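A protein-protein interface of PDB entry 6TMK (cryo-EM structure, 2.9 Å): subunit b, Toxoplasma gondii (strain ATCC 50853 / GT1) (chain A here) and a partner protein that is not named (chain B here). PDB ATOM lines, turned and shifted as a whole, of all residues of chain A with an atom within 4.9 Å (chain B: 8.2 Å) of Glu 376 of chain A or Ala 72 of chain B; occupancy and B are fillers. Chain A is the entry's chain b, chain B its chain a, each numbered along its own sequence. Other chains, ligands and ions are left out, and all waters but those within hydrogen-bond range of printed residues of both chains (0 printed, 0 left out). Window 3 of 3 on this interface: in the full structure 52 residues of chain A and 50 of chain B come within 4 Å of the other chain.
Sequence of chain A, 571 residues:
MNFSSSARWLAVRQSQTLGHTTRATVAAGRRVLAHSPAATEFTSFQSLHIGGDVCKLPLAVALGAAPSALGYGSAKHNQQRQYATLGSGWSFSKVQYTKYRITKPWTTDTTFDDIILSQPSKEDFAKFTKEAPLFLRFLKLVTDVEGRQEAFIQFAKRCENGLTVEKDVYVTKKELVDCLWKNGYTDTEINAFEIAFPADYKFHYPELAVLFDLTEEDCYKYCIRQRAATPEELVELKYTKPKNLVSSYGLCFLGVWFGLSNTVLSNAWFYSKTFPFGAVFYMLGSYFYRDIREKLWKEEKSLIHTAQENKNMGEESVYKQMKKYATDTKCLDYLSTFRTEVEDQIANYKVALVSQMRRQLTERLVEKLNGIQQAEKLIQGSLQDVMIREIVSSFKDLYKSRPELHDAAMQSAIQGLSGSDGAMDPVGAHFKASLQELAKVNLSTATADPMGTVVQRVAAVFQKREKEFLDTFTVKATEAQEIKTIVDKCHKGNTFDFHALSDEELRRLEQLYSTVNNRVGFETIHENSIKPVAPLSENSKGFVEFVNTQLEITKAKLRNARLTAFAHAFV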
ATOM      1  N   ILE A 372      30.008 -16.879  13.118  1.00  0.00           N
ATOM      2  CA  ILE A 372      29.864 -17.541  11.827  1.00  0.00           C
ATOM      3  C   ILE A 372      28.523 -18.262  11.752  1.00  0.00           C
ATOM      4  O   ILE A 372      27.880 -18.298  10.693  1.00  0.00           O
ATOM      5  CB  ILE A 372      31.044 -18.500  11.575  1.00  0.00           C
ATOM      6  CG1 ILE A 372      31.165 -18.801  10.082  1.00  0.00           C
ATOM      7  CG2 ILE A 372      30.865 -19.794  12.342  1.00  0.00           C
ATOM      8  CD1 ILE A 372      32.380 -19.625   9.727  1.00  0.00           C
ATOM      9  N   GLN A 373      28.068 -18.837  12.869  1.00  0.00           N
ATOM     10  CA  GLN A 373      26.751 -19.465  12.889  1.00  0.00           C
ATOM     11  C   GLN A 373      25.660 -18.435  12.621  1.00  0.00           C
ATOM     12  O   GLN A 373      24.740 -18.676  11.826  1.00  0.00           O
ATOM     13  CB  GLN A 373      26.525 -20.160  14.231  1.00  0.00           C
ATOM     14  CG  GLN A 373      25.066 -20.431  14.556  1.00  0.00           C
ATOM     15  CD  GLN A 373      24.897 -21.422  15.690  1.00  0.00           C
ATOM     16  OE1 GLN A 373      25.875 -21.890  16.272  1.00  0.00           O
ATOM     17  NE2 GLN A 373      23.650 -21.744  16.014  1.00  0.00           N
ATOM     18  N   GLN A 374      25.746 -17.275  13.279  1.00  0.00           N
ATOM     19  CA  GLN A 374      24.745 -16.236  13.053  1.00  0.00           C
ATOM     20  C   GLN A 374      24.770 -15.763  11.605  1.00  0.00           C
ATOM     21  O   GLN A 374      23.717 -15.506  11.004  1.00  0.00           O
ATOM     22  CB  GLN A 374      24.981 -15.066  14.007  1.00  0.00           C
ATOM     23  CG  GLN A 374      24.679 -15.389  15.459  1.00  0.00           C
ATOM     24  CD  GLN A 374      23.203 -15.635  15.704  1.00  0.00           C
ATOM     25  OE1 GLN A 374      22.347 -14.965  15.127  1.00  0.00           O
ATOM     26  NE2 GLN A 374      22.899 -16.604  16.559  1.00  0.00           N
ATOM     27  N   ALA A 375      25.967 -15.640  11.027  1.00  0.00           N
ATOM     28  CA  ALA A 375      26.075 -15.213   9.635  1.00  0.00           C
ATOM     29  C   ALA A 375      25.420 -16.226   8.706  1.00  0.00           C
ATOM     30  O   ALA A 375      24.674 -15.855   7.794  1.00  0.00           O
ATOM     31  CB  ALA A 375      27.543 -15.007   9.264  1.00  0.00           C
ATOM     32  N   GLU A 376      25.711 -17.515   8.905  1.00  0.00           N
ATOM     33  CA  GLU A 376      25.067 -18.555   8.108  1.00  0.00           C
ATOM     34  C   GLU A 376      23.549 -18.482   8.231  1.00  0.00           C
ATOM     35  O   GLU A 376      22.823 -18.612   7.232  1.00  0.00           O
ATOM     36  CB  GLU A 376      25.577 -19.931   8.538  1.00  0.00           C
ATOM     37  CG  GLU A 376      24.690 -21.087   8.104  1.00  0.00           C
ATOM     38  CD  GLU A 376      25.404 -22.425   8.160  1.00  0.00           C
ATOM     39  OE1 GLU A 376      26.585 -22.456   8.564  1.00  0.00           O
ATOM     40  OE2 GLU A 376      24.783 -23.446   7.797  1.00  0.00           O
ATOM     41  N   LYS A 377      23.050 -18.281   9.452  1.00  0.00           N
ATOM     42  CA  LYS A 377      21.607 -18.212   9.660  1.00  0.00           C
ATOM     43  C   LYS A 377      21.002 -17.056   8.874  1.00  0.00           C
ATOM     44  O   LYS A 377      19.990 -17.221   8.181  1.00  0.00           O
ATOM     45  CB  LYS A 377      21.300 -18.069  11.150  1.00  0.00           C
ATOM     46  CG  LYS A 377      19.925 -18.575  11.547  1.00  0.00           C
ATOM     47  CD  LYS A 377      19.828 -18.797  13.046  1.00  0.00           C
ATOM     48  CE  LYS A 377      20.380 -20.158  13.441  1.00  0.00           C
ATOM     49  NZ  LYS A 377      19.358 -21.233  13.313  1.00  0.00           N
ATOM     50  N   LEU A 378      21.602 -15.869   8.983  1.00  0.00           N
ATOM     51  CA  LEU A 378      21.049 -14.717   8.279  1.00  0.00           C
ATOM     52  C   LEU A 378      21.178 -14.883   6.771  1.00  0.00           C
ATOM     53  O   LEU A 378      20.310 -14.422   6.017  1.00  0.00           O
ATOM     54  CB  LEU A 378      21.751 -13.437   8.730  1.00  0.00           C
ATOM     55  CG  LEU A 378      21.096 -12.690   9.891  1.00  0.00           C
ATOM     56  CD1 LEU A 378      20.880 -13.618  11.076  1.00  0.00           C
ATOM     57  CD2 LEU A 378      21.942 -11.492  10.289  1.00  0.00           C
ATOM     58  N   ILE A 379      22.226 -15.574   6.321  1.00  0.00           N
ATOM     59  CA  ILE A 379      22.372 -15.886   4.903  1.00  0.00           C
ATOM     60  C   ILE A 379      21.182 -16.702   4.426  1.00  0.00           C
ATOM     61  O   ILE A 379      20.530 -16.360   3.433  1.00  0.00           O
ATOM     62  CB  ILE A 379      23.699 -16.627   4.656  1.00  0.00           C
ATOM     63  CG1 ILE A 379      24.850 -15.626   4.537  1.00  0.00           C
ATOM     64  CG2 ILE A 379      23.607 -17.495   3.398  1.00  0.00           C
ATOM     65  CD1 ILE A 379      26.227 -16.262   4.524  1.00  0.00           C
ATOM     66  N   GLN A 380      20.883 -17.801   5.125  1.00  0.00           N
ATOM     67  CA  GLN A 380      19.814 -18.681   4.662  1.00  0.00           C
ATOM     68  C   GLN A 380      18.456 -17.995   4.771  1.00  0.00           C
ATOM     69  O   GLN A 380      17.579 -18.188   3.916  1.00  0.00           O
ATOM     70  CB  GLN A 380      19.834 -19.995   5.448  1.00  0.00           C
ATOM     71  CG  GLN A 380      19.055 -19.985   6.754  1.00  0.00           C
ATOM     72  CD  GLN A 380      19.113 -21.319   7.471  1.00  0.00           C
ATOM     73  OE1 GLN A 380      19.823 -22.231   7.051  1.00  0.00           O
ATOM     74  NE2 GLN A 380      18.364 -21.439   8.559  1.00  0.00           N
ATOM     75  N   PHE A 469      30.381 -12.540   3.138  1.00  0.00           N
ATOM     76  CA  PHE A 469      30.616 -13.345   4.331  1.00  0.00           C
ATOM     77  C   PHE A 469      32.085 -13.740   4.422  1.00  0.00           C
ATOM     78  O   PHE A 469      32.729 -13.548   5.465  1.00  0.00           O
ATOM     79  CB  PHE A 469      29.707 -14.577   4.292  1.00  0.00           C
ATOM     80  CG  PHE A 469      30.127 -15.684   5.212  1.00  0.00           C
ATOM     81  CD1 PHE A 469      29.633 -15.754   6.502  1.00  0.00           C
ATOM     82  CD2 PHE A 469      30.982 -16.680   4.771  1.00  0.00           C
ATOM     83  CE1 PHE A 469      30.003 -16.783   7.343  1.00  0.00           C
ATOM     84  CE2 PHE A 469      31.360 -17.709   5.610  1.00  0.00           C
ATOM     85  CZ  PHE A 469      30.871 -17.759   6.897  1.00  0.00           C
ATOM     86  N   TRP B  67      29.650 -28.234  16.542  1.00  0.00           N
ATOM     87  CA  TRP B  67      29.794 -27.189  15.535  1.00  0.00           C
ATOM     88  C   TRP B  67      29.991 -27.763  14.140  1.00  0.00           C
ATOM     89  O   TRP B  67      29.503 -27.179  13.164  1.00  0.00           O
ATOM     90  CB  TRP B  67      30.967 -26.277  15.896  1.00  0.00           C
ATOM     91  CG  TRP B  67      30.895 -25.749  17.293  1.00  0.00           C
ATOM     92  CD1 TRP B  67      31.467 -26.295  18.405  1.00  0.00           C
ATOM     93  CD2 TRP B  67      30.212 -24.569  17.731  1.00  0.00           C
ATOM     94  NE1 TRP B  67      31.181 -25.529  19.508  1.00  0.00           N
ATOM     95  CE2 TRP B  67      30.413 -24.463  19.121  1.00  0.00           C
ATOM     96  CE3 TRP B  67      29.451 -23.592  17.082  1.00  0.00           C
ATOM     97  CZ2 TRP B  67      29.880 -23.419  19.874  1.00  0.00           C
ATOM     98  CZ3 TRP B  67      28.923 -22.556  17.831  1.00  0.00           C
ATOM     99  CH2 TRP B  67      29.139 -22.478  19.212  1.00  0.00           C
ATOM    100  N   GLU B  68      30.639 -28.926  14.024  1.00  0.00           N
ATOM    101  CA  GLU B  68      30.735 -29.582  12.725  1.00  0.00           C
ATOM    102  C   GLU B  68      29.353 -29.864  12.156  1.00  0.00           C
ATOM    103  O   GLU B  68      29.155 -29.800  10.937  1.00  0.00           O
ATOM    104  CB  GLU B  68      31.538 -30.877  12.848  1.00  0.00           C
ATOM    105  CG  GLU B  68      33.009 -30.721  12.499  1.00  0.00           C
ATOM    106  CD  GLU B  68      33.887 -31.727  13.215  1.00  0.00           C
ATOM    107  OE1 GLU B  68      33.403 -32.841  13.506  1.00  0.00           O
ATOM    108  OE2 GLU B  68      35.062 -31.402  13.489  1.00  0.00           O
ATOM    109  N   SER B  69      28.388 -30.175  13.021  1.00  0.00           N
ATOM    110  CA  SER B  69      27.030 -30.438  12.566  1.00  0.00           C
ATOM    111  C   SER B  69      26.284 -29.131  12.329  1.00  0.00           C
ATOM    112  O   SER B  69      25.639 -28.953  11.290  1.00  0.00           O
ATOM    113  CB  SER B  69      26.292 -31.302  13.590  1.00  0.00           C
ATOM    114  OG  SER B  69      26.896 -32.577  13.711  1.00  0.00           O
ATOM    115  N   GLN B  70      26.364 -28.204  13.286  1.00  0.00           N
ATOM    116  CA  GLN B  70      25.590 -26.973  13.213  1.00  0.00           C
ATOM    117  C   GLN B  70      26.078 -26.024  12.127  1.00  0.00           C
ATOM    118  O   GLN B  70      25.378 -25.051  11.830  1.00  0.00           O
ATOM    119  CB  GLN B  70      25.609 -26.260  14.565  1.00  0.00           C
ATOM    120  CG  GLN B  70      24.544 -26.756  15.527  1.00  0.00           C
ATOM    121  CD  GLN B  70      24.663 -26.137  16.905  1.00  0.00           C
ATOM    122  OE1 GLN B  70      24.579 -26.833  17.917  1.00  0.00           O
ATOM    123  NE2 GLN B  70      24.858 -24.825  16.952  1.00  0.00           N
ATOM    124  N   ILE B  71      27.243 -26.273  11.529  1.00  0.00           N
ATOM    125  CA  ILE B  71      27.779 -25.390  10.504  1.00  0.00           C
ATOM    126  C   ILE B  71      27.837 -26.153   9.189  1.00  0.00           C
ATOM    127  O   ILE B  71      28.074 -27.365   9.157  1.00  0.00           O
ATOM    128  CB  ILE B  71      29.178 -24.853  10.882  1.00  0.00           C
ATOM    129  CG1 ILE B  71      29.145 -24.160  12.248  1.00  0.00           C
ATOM    130  CG2 ILE B  71      29.684 -23.891   9.818  1.00  0.00           C
ATOM    131  CD1 ILE B  71      28.056 -23.119  12.399  1.00  0.00           C
ATOM    132  N   ALA B  72      27.617 -25.424   8.094  1.00  0.00           N
ATOM    133  CA  ALA B  72      27.512 -26.020   6.770  1.00  0.00           C
ATOM    134  C   ALA B  72      28.779 -25.882   5.939  1.00  0.00           C
ATOM    135  O   ALA B  72      28.963 -26.650   4.988  1.00  0.00           O
ATOM    136  CB  ALA B  72      26.341 -25.395   6.002  1.00  0.00           C
ATOM    137  N   HIS B  73      29.653 -24.930   6.269  1.00  0.00           N
ATOM    138  CA  HIS B  73      30.858 -24.721   5.473  1.00  0.00           C
ATOM    139  C   HIS B  73      31.845 -25.864   5.675  1.00  0.00           C
ATOM    140  O   HIS B  73      32.169 -26.596   4.732  1.00  0.00           O
ATOM    141  CB  HIS B  73      31.495 -23.379   5.838  1.00  0.00           C
ATOM    142  CG  HIS B  73      30.777 -22.198   5.266  1.00  0.00           C
ATOM    143  ND1 HIS B  73      30.298 -22.172   3.974  1.00  0.00           N
ATOM    144  CD2 HIS B  73      30.443 -21.006   5.814  1.00  0.00           C
ATOM    145  CE1 HIS B  73      29.708 -21.012   3.748  1.00  0.00           C
ATOM    146  NE2 HIS B  73      29.781 -20.287   4.849  1.00  0.00           N
ATOM    147  N   LYS B  74      32.332 -26.034   6.903  1.00  0.00           N
ATOM    148  CA  LYS B  74      33.199 -27.159   7.251  1.00  0.00           C
ATOM    149  C   LYS B  74      34.466 -27.186   6.399  1.00  0.00           C
ATOM    150  O   LYS B  74      34.989 -28.256   6.079  1.00  0.00           O
ATOM    151  CB  LYS B  74      32.446 -28.485   7.132  1.00  0.00           C
ATOM    152  CG  LYS B  74      31.083 -28.473   7.809  1.00  0.00           C
ATOM    153  CD  LYS B  74      30.433 -29.847   7.794  1.00  0.00           C
ATOM    154  CE  LYS B  74      29.846 -30.173   6.431  1.00  0.00           C
ATOM    155  NZ  LYS B  74      28.528 -29.512   6.222  1.00  0.00           N
ATOM    156  N   ASP B  75      34.965 -26.011   6.029  1.00  0.00           N
ATOM    157  CA  ASP B  75      36.206 -25.876   5.275  1.00  0.00           C
ATOM    158  C   ASP B  75      37.228 -25.016   5.997  1.00  0.00           C
ATOM    159  O   ASP B  75      38.424 -25.313   5.948  1.00  0.00           O
ATOM    160  CB  ASP B  75      35.922 -25.278   3.889  1.00  0.00           C
ATOM    161  CG  ASP B  75      35.040 -24.045   3.956  1.00  0.00           C
ATOM    162  OD1 ASP B  75      34.888 -23.480   5.058  1.00  0.00           O
ATOM    163  OD2 ASP B  75      34.502 -23.640   2.904  1.00  0.00           O
ATOM    164  N   LEU B  77      36.424 -24.154   9.367  1.00  0.00           N
ATOM    165  CA  LEU B  77      36.292 -24.753  10.689  1.00  0.00           C
ATOM    166  C   LEU B  77      37.366 -25.806  10.929  1.00  0.00           C
ATOM    167  O   LEU B  77      37.904 -25.914  12.036  1.00  0.00           O
ATOM    168  CB  LEU B  77      34.898 -25.366  10.841  1.00  0.00           C
ATOM    169  CG  LEU B  77      34.549 -25.963  12.205  1.00  0.00           C
ATOM    170  CD1 LEU B  77      34.433 -24.875  13.260  1.00  0.00           C
ATOM    171  CD2 LEU B  77      33.257 -26.762  12.116  1.00  0.00           C
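The side-chain amino group (NZ) of Lys 74 of chain B sits at hydrogen-bond distance from the backbone carbonyl oxygen (O) of Ala 72 of chain B, at 3.1 Å.
Printed residues of chain A that touch a printed residue of chain B: Gln 373, Glu 376 and Phe 469.
Of the 10 printed residues of chain B, 5 touch a printed residue of chain A.
Hydrophobic or aromatic side chains of chain B that line the printed part of chain A: Trp 67, Ile 71, Ala 72 and His 73.
Among the printed residues, no Asp or Glu carboxylate lies within 4 Å of a Lys or Arg side-chain nitrogen of the other chain.
OE1 of Gln 373 of chain A is in hydrogen-bond range of NE2 of Gln 70 of chain B, at 3.2 Å.
OE1 of Glu 376 of chain A lies within hydrogen-bond range of N of Ala 72 of chain B, at 3.2 Å.
Gln 373 of chain A touches Trp 67 of chain B.
CB of Gln 373 of chain A touches CD1 of Ile 71 of chain B, at 3.8 Å.
Ile 71 of chain B touches Glu 376 of chain A (CG2 to OE1, 3.6 Å).
His 73 of chain B touches Phe 469 of chain A (NE2 to CE2, 3.1 Å).
Printed residues of chain B within 4 Å of Glu 376 of chain A: Ile 71 and Ala 72.
Printed residues of chain A within 4 Å of Ala 72 of chain B: Glu 376.
No residue of chain B comes within 4 Å of Ala 375 of chain A.
Of the printed residues of chain A, Ile 71 of chain B touches Gln 373 and Glu 376.
Of the printed residues of chain B, Phe 469 of chain A touches His 73 (3.1 Å).
Printed residues of chain A within 4 Å of Trp 67 of chain B: Gln 373.
Of the printed residues of chain B, Gln 373 of chain A touches Trp 67, Gln 70 and Ile 71.
Printed residues of chain A within 4 Å of Gln 70 of chain B: Gln 373 (3.2 Å).
Ser 69 of chain B touches none of the printed residues of chain A.
The nearest printed residue of chain A that does not touch Trp 67 of chain B is Ile 372 of chain A (6.2 Å).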
